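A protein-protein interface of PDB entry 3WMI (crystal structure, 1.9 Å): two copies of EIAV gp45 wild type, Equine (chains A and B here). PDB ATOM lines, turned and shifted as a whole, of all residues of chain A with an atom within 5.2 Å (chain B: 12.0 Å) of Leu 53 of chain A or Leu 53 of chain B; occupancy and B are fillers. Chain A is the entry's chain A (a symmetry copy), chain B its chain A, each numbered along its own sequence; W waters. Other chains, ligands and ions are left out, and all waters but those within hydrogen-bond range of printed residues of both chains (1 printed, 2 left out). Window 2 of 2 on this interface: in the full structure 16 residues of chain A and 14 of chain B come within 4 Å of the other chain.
The side-chain amino group of Lys 54 of chain B is in salt-bridge range of the side-chain carboxylate of Asp 49 of chain A (3.7 Å).
The side-chain amino group (NZ) of Lys 54 of chain B lies within hydrogen-bond range of the side-chain amide oxygen (OE1) of Gln 51 of chain B, 2.9 Å away.
Among the printed residues, pairs that only touch across the chains: Gln 56 of chain A with Gln 57 of chain B (3.3 Å), Val 50 of chain A with Val 50 of chain B (3.7 Å), Asp 49 of chain A with Val 50 of chain B (3.8 Å), Leu 53 of chain A with Leu 53 of chain B (3.8 Å) and Gln 57 of chain A with Gln 57 of chain B (3.9 Å).
Of the printed residues of chain B, Leu 53 of chain A touches Leu 53 (3.8 Å).
Leu 53 of chain B touches just one residue of chain A: Leu 53.
Of chain B, only Val 50 (3.7 Å) comes within 4 Å of Val 50 of chain A.
No residue of chain B comes within 4 Å of Gln 51 of chain A.
No residue of chain B comes within 4 Å of Lys 54 of chain A.
No residue of chain B comes within 4 Å of Glu 55 of chain A.
Of chain B, only Gln 57 (3.9 Å) comes within 4 Å of Gln 57 of chain A.
Printed residues of chain A within 4 Å of Gln 57 of chain B: Gln 56 and Gln 57.
Of the printed residues of chain A, Lys 54 of chain B touches Asp 49.
Printed residues of chain A within 4 Å of Val 50 of chain B: Asp 49 (3.8 Å) and Val 50 (3.7 Å).
The nearest residue of chain B that does not touch Leu 53 of chain A is Gln 57 of chain B (4.1 Å).
The nearest printed residue of chain A that does not touch Leu 53 of chain B is Gln 56 of chain A (6.3 Å).
The nearest printed residue of chain A that does not touch Gln 57 of chain B is Leu 53 of chain A (4.1 Å).
Of the 9 printed residues of chain A, 5 touch a printed residue of chain B.
Printed residues of chain A that touch a printed residue of chain B: Asp 49, Val 50, Leu 53, Gln 56 and Gln 57.
Of the 15 printed residues of chain B, 4 touch a printed residue of chain A.
Hydrophobic or aromatic side chains of chain B that line the printed part of chain A: Val 50 and Leu 53.
Among the printed residues, Asp or Glu carboxylates within 4 Å of a Lys or Arg side-chain nitrogen of the other chain: Asp 49 of chain A with Lys 54 of chain B (3.7 Å).
Asp 49 of chain A touches Val 50 of chain B, but with the chains exchanged Val 50 of chain A does not touch Asp 49 of chain B (7.6 Å).
Val 50 of chain A touches its own counterpart, Val 50 of chain B.
Gln 56 of chain A touches Gln 57 of chain B, but with the chains exchanged Gln 57 of chain A does not touch Gln 56 of chain B (7.8 Å).
Gln 57 of chain B touches its own counterpart, Gln 57 of chain A.
Of the 6 pairs that touch across the chains among the printed residues, 3 have their exchanged pair printed and touching as well.
Water W1 bridges ND1 of His 47 of chain B (2.7 Å) and OD2 of Asp 49 of chain A (3.4 Å).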
ATOM      1  N   ASP A  49     -15.510 -30.486  -6.796  1.00  0.00           N
ATOM      2  CA  ASP A  49     -15.075 -30.853  -8.144  1.00  0.00           C
ATOM      3  C   ASP A  49     -14.003 -29.889  -8.633  1.00  0.00           C
ATOM      4  O   ASP A  49     -12.990 -30.299  -9.228  1.00  0.00           O
ATOM      5  CB  ASP A  49     -16.249 -30.858  -9.127  1.00  0.00           C
ATOM      6  CG  ASP A  49     -17.256 -31.948  -8.831  1.00  0.00           C
ATOM      7  OD1 ASP A  49     -16.878 -32.966  -8.205  1.00  0.00           O
ATOM      8  OD2 ASP A  49     -18.431 -31.775  -9.217  1.00  0.00           O
ATOM      9  N   VAL A  50     -14.234 -28.607  -8.397  1.00  0.00           N
ATOM     10  CA  VAL A  50     -13.291 -27.576  -8.814  1.00  0.00           C
ATOM     11  C   VAL A  50     -11.935 -27.733  -8.111  1.00  0.00           C
ATOM     12  O   VAL A  50     -10.881 -27.634  -8.742  1.00  0.00           O
ATOM     13  CB  VAL A  50     -13.878 -26.166  -8.605  1.00  0.00           C
ATOM     14  CG1 VAL A  50     -12.799 -25.114  -8.723  1.00  0.00           C
ATOM     15  CG2 VAL A  50     -14.998 -25.913  -9.615  1.00  0.00           C
ATOM     16  N   GLN A  51     -11.959 -28.014  -6.817  1.00  0.00           N
ATOM     17  CA  GLN A  51     -10.724 -28.258  -6.075  1.00  0.00           C
ATOM     18  C   GLN A  51      -9.879 -29.386  -6.673  1.00  0.00           C
ATOM     19  O   GLN A  51      -8.647 -29.277  -6.766  1.00  0.00           O
ATOM     20  CB  GLN A  51     -11.026 -28.555  -4.607  1.00  0.00           C
ATOM     21  CG  GLN A  51     -11.592 -27.369  -3.852  1.00  0.00           C
ATOM     22  CD  GLN A  51     -10.639 -26.204  -3.799  1.00  0.00           C
ATOM     23  OE1 GLN A  51     -10.910 -25.146  -4.361  1.00  0.00           O
ATOM     24  NE2 GLN A  51      -9.517 -26.382  -3.114  1.00  0.00           N
ATOM     25  N   LEU A  52     -10.536 -30.460  -7.099  1.00  0.00           N
ATOM     26  CA  LEU A  52      -9.820 -31.584  -7.709  1.00  0.00           C
ATOM     27  C   LEU A  52      -9.228 -31.196  -9.059  1.00  0.00           C
ATOM     28  O   LEU A  52      -8.086 -31.545  -9.378  1.00  0.00           O
ATOM     29  CB  LEU A  52     -10.748 -32.793  -7.848  1.00  0.00           C
ATOM     30  CG  LEU A  52     -10.118 -34.045  -8.460  1.00  0.00           C
ATOM     31  CD1 LEU A  52      -8.947 -34.519  -7.593  1.00  0.00           C
ATOM     32  CD2 LEU A  52     -11.157 -35.141  -8.634  1.00  0.00           C
ATOM     33  N   LEU A  53     -10.007 -30.470  -9.852  1.00  0.00           N
ATOM     34  CA  LEU A  53      -9.538 -29.959 -11.138  1.00  0.00           C
ATOM     35  C   LEU A  53      -8.321 -29.060 -10.968  1.00  0.00           C
ATOM     36  O   LEU A  53      -7.367 -29.144 -11.744  1.00  0.00           O
ATOM     37  CB  LEU A  53     -10.659 -29.215 -11.863  1.00  0.00           C
ATOM     38  CG  LEU A  53     -11.732 -30.105 -12.470  1.00  0.00           C
ATOM     39  CD1 LEU A  53     -12.923 -29.249 -12.897  1.00  0.00           C
ATOM     40  CD2 LEU A  53     -11.158 -30.903 -13.652  1.00  0.00           C
ATOM     41  N   LYS A  54      -8.345 -28.214  -9.945  1.00  0.00           N
ATOM     42  CA  LYS A  54      -7.202 -27.355  -9.649  1.00  0.00           C
ATOM     43  C   LYS A  54      -5.974 -28.184  -9.261  1.00  0.00           C
ATOM     44  O   LYS A  54      -4.852 -27.856  -9.642  1.00  0.00           O
ATOM     45  CB  LYS A  54      -7.539 -26.346  -8.556  1.00  0.00           C
ATOM     46  CG  LYS A  54      -8.508 -25.274  -9.005  1.00  0.00           C
ATOM     47  CD  LYS A  54      -8.499 -24.080  -8.063  1.00  0.00           C
ATOM     48  CE  LYS A  54      -9.291 -24.366  -6.825  1.00  0.00           C
ATOM     49  NZ  LYS A  54      -9.252 -23.249  -5.831  1.00  0.00           N
ATOM     50  N   GLU A  55      -6.193 -29.261  -8.513  1.00  0.00           N
ATOM     51  CA  GLU A  55      -5.104 -30.170  -8.145  1.00  0.00           C
ATOM     52  C   GLU A  55      -4.546 -30.912  -9.356  1.00  0.00           C
ATOM     53  O   GLU A  55      -3.336 -31.129  -9.459  1.00  0.00           O
ATOM     54  CB  GLU A  55      -5.563 -31.173  -7.082  1.00  0.00           C
ATOM     55  CG  GLU A  55      -5.693 -30.578  -5.694  1.00  0.00           C
ATOM     56  CD  GLU A  55      -4.375 -30.019  -5.174  1.00  0.00           C
ATOM     57  OE1 GLU A  55      -3.342 -30.715  -5.293  1.00  0.00           O
ATOM     58  OE2 GLU A  55      -4.374 -28.883  -4.655  1.00  0.00           O
ATOM     59  N   GLN A  56      -5.429 -31.298 -10.270  1.00  0.00           N
ATOM     60  CA  GLN A  56      -5.036 -32.020 -11.476  1.00  0.00           C
ATOM     61  C   GLN A  56      -4.338 -31.121 -12.498  1.00  0.00           C
ATOM     62  O   GLN A  56      -3.543 -31.589 -13.310  1.00  0.00           O
ATOM     63  CB  GLN A  56      -6.260 -32.668 -12.117  1.00  0.00           C
ATOM     64  CG  GLN A  56      -6.870 -33.793 -11.298  1.00  0.00           C
ATOM     65  CD  GLN A  56      -8.242 -34.197 -11.800  1.00  0.00           C
ATOM     66  OE1 GLN A  56      -8.963 -33.394 -12.391  1.00  0.00           O
ATOM     67  NE2 GLN A  56      -8.608 -35.448 -11.573  1.00  0.00           N
ATOM     68  N   GLN A  57      -4.653 -29.832 -12.462  1.00  0.00           N
ATOM     69  CA  GLN A  57      -4.118 -28.881 -13.433  1.00  0.00           C
ATOM     70  C   GLN A  57      -2.689 -28.475 -13.089  1.00  0.00           C
ATOM     71  O   GLN A  57      -2.290 -28.502 -11.926  1.00  0.00           O
ATOM     72  CB  GLN A  57      -5.016 -27.642 -13.514  1.00  0.00           C
ATOM     73  CG  GLN A  57      -4.587 -26.614 -14.558  1.00  0.00           C
ATOM     74  CD  GLN A  57      -4.703 -27.140 -15.977  1.00  0.00           C
ATOM     75  OE1 GLN A  57      -5.450 -28.085 -16.244  1.00  0.00           O
ATOM     76  NE2 GLN A  57      -3.954 -26.536 -16.896  1.00  0.00           N
ATOM     77  N   VAL B  43     -25.677 -21.619 -10.798  1.00  0.00           N
ATOM     78  CA  VAL B  43     -25.163 -22.886 -10.279  1.00  0.00           C
ATOM     79  C   VAL B  43     -25.212 -23.988 -11.349  1.00  0.00           C
ATOM     80  O   VAL B  43     -24.254 -24.755 -11.518  1.00  0.00           O
ATOM     81  CB  VAL B  43     -25.927 -23.303  -8.980  1.00  0.00           C
ATOM     82  CG1 VAL B  43     -25.762 -24.800  -8.686  1.00  0.00           C
ATOM     83  CG2 VAL B  43     -25.441 -22.464  -7.795  1.00  0.00           C
ATOM     84  N   LEU B  44     -26.323 -24.051 -12.079  1.00  0.00           N
ATOM     85  CA  LEU B  44     -26.465 -25.000 -13.181  1.00  0.00           C
ATOM     86  C   LEU B  44     -25.456 -24.727 -14.303  1.00  0.00           C
ATOM     87  O   LEU B  44     -24.870 -25.660 -14.868  1.00  0.00           O
ATOM     88  CB  LEU B  44     -27.895 -24.963 -13.738  1.00  0.00           C
ATOM     89  CG  LEU B  44     -29.013 -25.559 -12.878  1.00  0.00           C
ATOM     90  CD1 LEU B  44     -30.383 -25.374 -13.545  1.00  0.00           C
ATOM     91  CD2 LEU B  44     -28.789 -27.025 -12.567  1.00  0.00           C
ATOM     92  N   GLN B  45     -25.263 -23.457 -14.635  1.00  0.00           N
ATOM     93  CA  GLN B  45     -24.291 -23.090 -15.666  1.00  0.00           C
ATOM     94  C   GLN B  45     -22.865 -23.466 -15.267  1.00  0.00           C
ATOM     95  O   GLN B  45     -22.114 -24.022 -16.067  1.00  0.00           O
ATOM     96  CB  GLN B  45     -24.371 -21.593 -15.974  1.00  0.00           C
ATOM     97  CG  GLN B  45     -23.324 -21.106 -16.978  1.00  0.00           C
ATOM     98  CD  GLN B  45     -23.561 -21.655 -18.363  1.00  0.00           C
ATOM     99  OE1 GLN B  45     -24.703 -21.827 -18.777  1.00  0.00           O
ATOM    100  NE2 GLN B  45     -22.479 -21.948 -19.086  1.00  0.00           N
ATOM    101  N   THR B  46     -22.497 -23.161 -14.027  1.00  0.00           N
ATOM    102  CA  THR B  46     -21.170 -23.502 -13.521  1.00  0.00           C
ATOM    103  C   THR B  46     -20.954 -25.013 -13.535  1.00  0.00           C
ATOM    104  O   THR B  46     -19.879 -25.493 -13.896  1.00  0.00           O
ATOM    105  CB  THR B  46     -20.955 -22.956 -12.097  1.00  0.00           C
ATOM    106  OG1 THR B  46     -21.050 -21.527 -12.122  1.00  0.00           O
ATOM    107  CG2 THR B  46     -19.582 -23.348 -11.574  1.00  0.00           C
ATOM    108  N   HIS B  47     -21.990 -25.755 -13.163  1.00  0.00           N
ATOM    109  CA  HIS B  47     -21.948 -27.218 -13.178  1.00  0.00           C
ATOM    110  C   HIS B  47     -21.655 -27.739 -14.580  1.00  0.00           C
ATOM    111  O   HIS B  47     -20.828 -28.638 -14.762  1.00  0.00           O
ATOM    112  CB  HIS B  47     -23.291 -27.772 -12.699  1.00  0.00           C
ATOM    113  CG  HIS B  47     -23.365 -29.270 -12.680  1.00  0.00           C
ATOM    114  ND1 HIS B  47     -22.562 -30.046 -11.873  1.00  0.00           N
ATOM    115  CD2 HIS B  47     -24.161 -30.132 -13.358  1.00  0.00           C
ATOM    116  CE1 HIS B  47     -22.860 -31.321 -12.056  1.00  0.00           C
ATOM    117  NE2 HIS B  47     -23.827 -31.400 -12.950  1.00  0.00           N
ATOM    118  N   ALA B  48     -22.346 -27.178 -15.565  1.00  0.00           N
ATOM    119  CA  ALA B  48     -22.106 -27.515 -16.970  1.00  0.00           C
ATOM    120  C   ALA B  48     -20.647 -27.290 -17.350  1.00  0.00           C
ATOM    121  O   ALA B  48     -20.011 -28.157 -17.971  1.00  0.00           O
ATOM    122  CB  ALA B  48     -23.014 -26.696 -17.874  1.00  0.00           C
ATOM    123  N   ASP B  49     -20.108 -26.127 -16.994  1.00  0.00           N
ATOM    124  CA  ASP B  49     -18.712 -25.829 -17.313  1.00  0.00           C
ATOM    125  C   ASP B  49     -17.790 -26.844 -16.651  1.00  0.00           C
ATOM    126  O   ASP B  49     -16.827 -27.338 -17.266  1.00  0.00           O
ATOM    127  CB  ASP B  49     -18.326 -24.416 -16.861  1.00  0.00           C
ATOM    128  CG  ASP B  49     -19.048 -23.337 -17.638  1.00  0.00           C
ATOM    129  OD1 ASP B  49     -19.473 -23.601 -18.788  1.00  0.00           O
ATOM    130  OD2 ASP B  49     -19.199 -22.226 -17.088  1.00  0.00           O
ATOM    131  N   VAL B  50     -18.076 -27.145 -15.394  1.00  0.00           N
ATOM    132  CA  VAL B  50     -17.274 -28.101 -14.641  1.00  0.00           C
ATOM    133  C   VAL B  50     -17.331 -29.503 -15.266  1.00  0.00           C
ATOM    134  O   VAL B  50     -16.307 -30.175 -15.405  1.00  0.00           O
ATOM    135  CB  VAL B  50     -17.685 -28.126 -13.156  1.00  0.00           C
ATOM    136  CG1 VAL B  50     -17.095 -29.329 -12.457  1.00  0.00           C
ATOM    137  CG2 VAL B  50     -17.247 -26.830 -12.472  1.00  0.00           C
ATOM    138  N   GLN B  51     -18.516 -29.928 -15.676  1.00  0.00           N
ATOM    139  CA  GLN B  51     -18.663 -31.216 -16.353  1.00  0.00           C
ATOM    140  C   GLN B  51     -17.784 -31.339 -17.600  1.00  0.00           C
ATOM    141  O   GLN B  51     -17.169 -32.388 -17.844  1.00  0.00           O
ATOM    142  CB  GLN B  51     -20.124 -31.472 -16.718  1.00  0.00           C
ATOM    143  CG  GLN B  51     -21.024 -31.669 -15.514  1.00  0.00           C
ATOM    144  CD  GLN B  51     -20.639 -32.871 -14.690  1.00  0.00           C
ATOM    145  OE1 GLN B  51     -20.226 -32.737 -13.542  1.00  0.00           O
ATOM    146  NE2 GLN B  51     -20.781 -34.057 -15.266  1.00  0.00           N
ATOM    147  N   LEU B  52     -17.702 -30.266 -18.380  1.00  0.00           N
ATOM    148  CA  LEU B  52     -16.868 -30.275 -19.585  1.00  0.00           C
ATOM    149  C   LEU B  52     -15.386 -30.345 -19.231  1.00  0.00           C
ATOM    150  O   LEU B  52     -14.616 -31.081 -19.858  1.00  0.00           O
ATOM    151  CB  LEU B  52     -17.164 -29.046 -20.446  1.00  0.00           C
ATOM    152  CG  LEU B  52     -16.368 -28.941 -21.748  1.00  0.00           C
ATOM    153  CD1 LEU B  52     -16.659 -30.153 -22.639  1.00  0.00           C
ATOM    154  CD2 LEU B  52     -16.679 -27.639 -22.466  1.00  0.00           C
ATOM    155  N   LEU B  53     -14.989 -29.578 -18.224  1.00  0.00           N
ATOM    156  CA  LEU B  53     -13.616 -29.609 -17.725  1.00  0.00           C
ATOM    157  C   LEU B  53     -13.229 -31.001 -17.246  1.00  0.00           C
ATOM    158  O   LEU B  53     -12.121 -31.470 -17.512  1.00  0.00           O
ATOM    159  CB  LEU B  53     -13.426 -28.583 -16.608  1.00  0.00           C
ATOM    160  CG  LEU B  53     -13.356 -27.135 -17.071  1.00  0.00           C
ATOM    161  CD1 LEU B  53     -13.462 -26.207 -15.863  1.00  0.00           C
ATOM    162  CD2 LEU B  53     -12.059 -26.890 -17.858  1.00  0.00           C
ATOM    163  N   LYS B  54     -14.146 -31.667 -16.554  1.00  0.00           N
ATOM    164  CA  LYS B  54     -13.906 -33.035 -16.104  1.00  0.00           C
ATOM    165  C   LYS B  54     -13.747 -33.987 -17.294  1.00  0.00           C
ATOM    166  O   LYS B  54     -12.916 -34.891 -17.264  1.00  0.00           O
ATOM    167  CB  LYS B  54     -15.016 -33.513 -15.175  1.00  0.00           C
ATOM    168  CG  LYS B  54     -15.004 -32.834 -13.822  1.00  0.00           C
ATOM    169  CD  LYS B  54     -15.826 -33.604 -12.802  1.00  0.00           C
ATOM    170  CE  LYS B  54     -17.290 -33.347 -12.986  1.00  0.00           C
ATOM    171  NZ  LYS B  54     -18.148 -34.140 -12.052  1.00  0.00           N
ATOM    172  N   GLU B  55     -14.539 -33.772 -18.339  1.00  0.00           N
ATOM    173  CA  GLU B  55     -14.424 -34.571 -19.563  1.00  0.00           C
ATOM    174  C   GLU B  55     -13.107 -34.317 -20.289  1.00  0.00           C
ATOM    175  O   GLU B  55     -12.500 -35.242 -20.835  1.00  0.00           O
ATOM    176  CB  GLU B  55     -15.601 -34.305 -20.505  1.00  0.00           C
ATOM    177  CG  GLU B  55     -16.899 -34.952 -20.063  1.00  0.00           C
ATOM    178  CD  GLU B  55     -16.792 -36.469 -19.975  1.00  0.00           C
ATOM    179  OE1 GLU B  55     -16.257 -37.086 -20.924  1.00  0.00           O
ATOM    180  OE2 GLU B  55     -17.237 -37.039 -18.957  1.00  0.00           O
ATOM    181  N   GLN B  56     -12.667 -33.064 -20.292  1.00  0.00           N
ATOM    182  CA  GLN B  56     -11.424 -32.676 -20.952  1.00  0.00           C
ATOM    183  C   GLN B  56     -10.184 -33.132 -20.183  1.00  0.00           C
ATOM    184  O   GLN B  56      -9.119 -33.331 -20.764  1.00  0.00           O
ATOM    185  CB  GLN B  56     -11.383 -31.161 -21.137  1.00  0.00           C
ATOM    186  CG  GLN B  56     -12.408 -30.627 -22.123  1.00  0.00           C
ATOM    187  CD  GLN B  56     -12.551 -29.120 -22.049  1.00  0.00           C
ATOM    188  OE1 GLN B  56     -12.309 -28.509 -21.009  1.00  0.00           O
ATOM    189  NE2 GLN B  56     -12.938 -28.510 -23.158  1.00  0.00           N
ATOM    190  N   GLN B  57     -10.324 -33.280 -18.871  1.00  0.00           N
ATOM    191  CA  GLN B  57      -9.198 -33.633 -18.010  1.00  0.00           C
ATOM    192  C   GLN B  57      -8.888 -35.126 -18.080  1.00  0.00           C
ATOM    193  O   GLN B  57      -9.768 -35.939 -18.358  1.00  0.00           O
ATOM    194  CB  GLN B  57      -9.484 -33.219 -16.564  1.00  0.00           C
ATOM    195  CG  GLN B  57      -8.335 -33.476 -15.591  1.00  0.00           C
ATOM    196  CD  GLN B  57      -7.115 -32.627 -15.892  1.00  0.00           C
ATOM    197  OE1 GLN B  57      -7.213 -31.582 -16.542  1.00  0.00           O
ATOM    198  NE2 GLN B  57      -5.950 -33.077 -15.429  1.00  0.00           N
HETATM  199  O   HOH W   1     -20.486 -29.355 -10.327  1.00  0.00           O
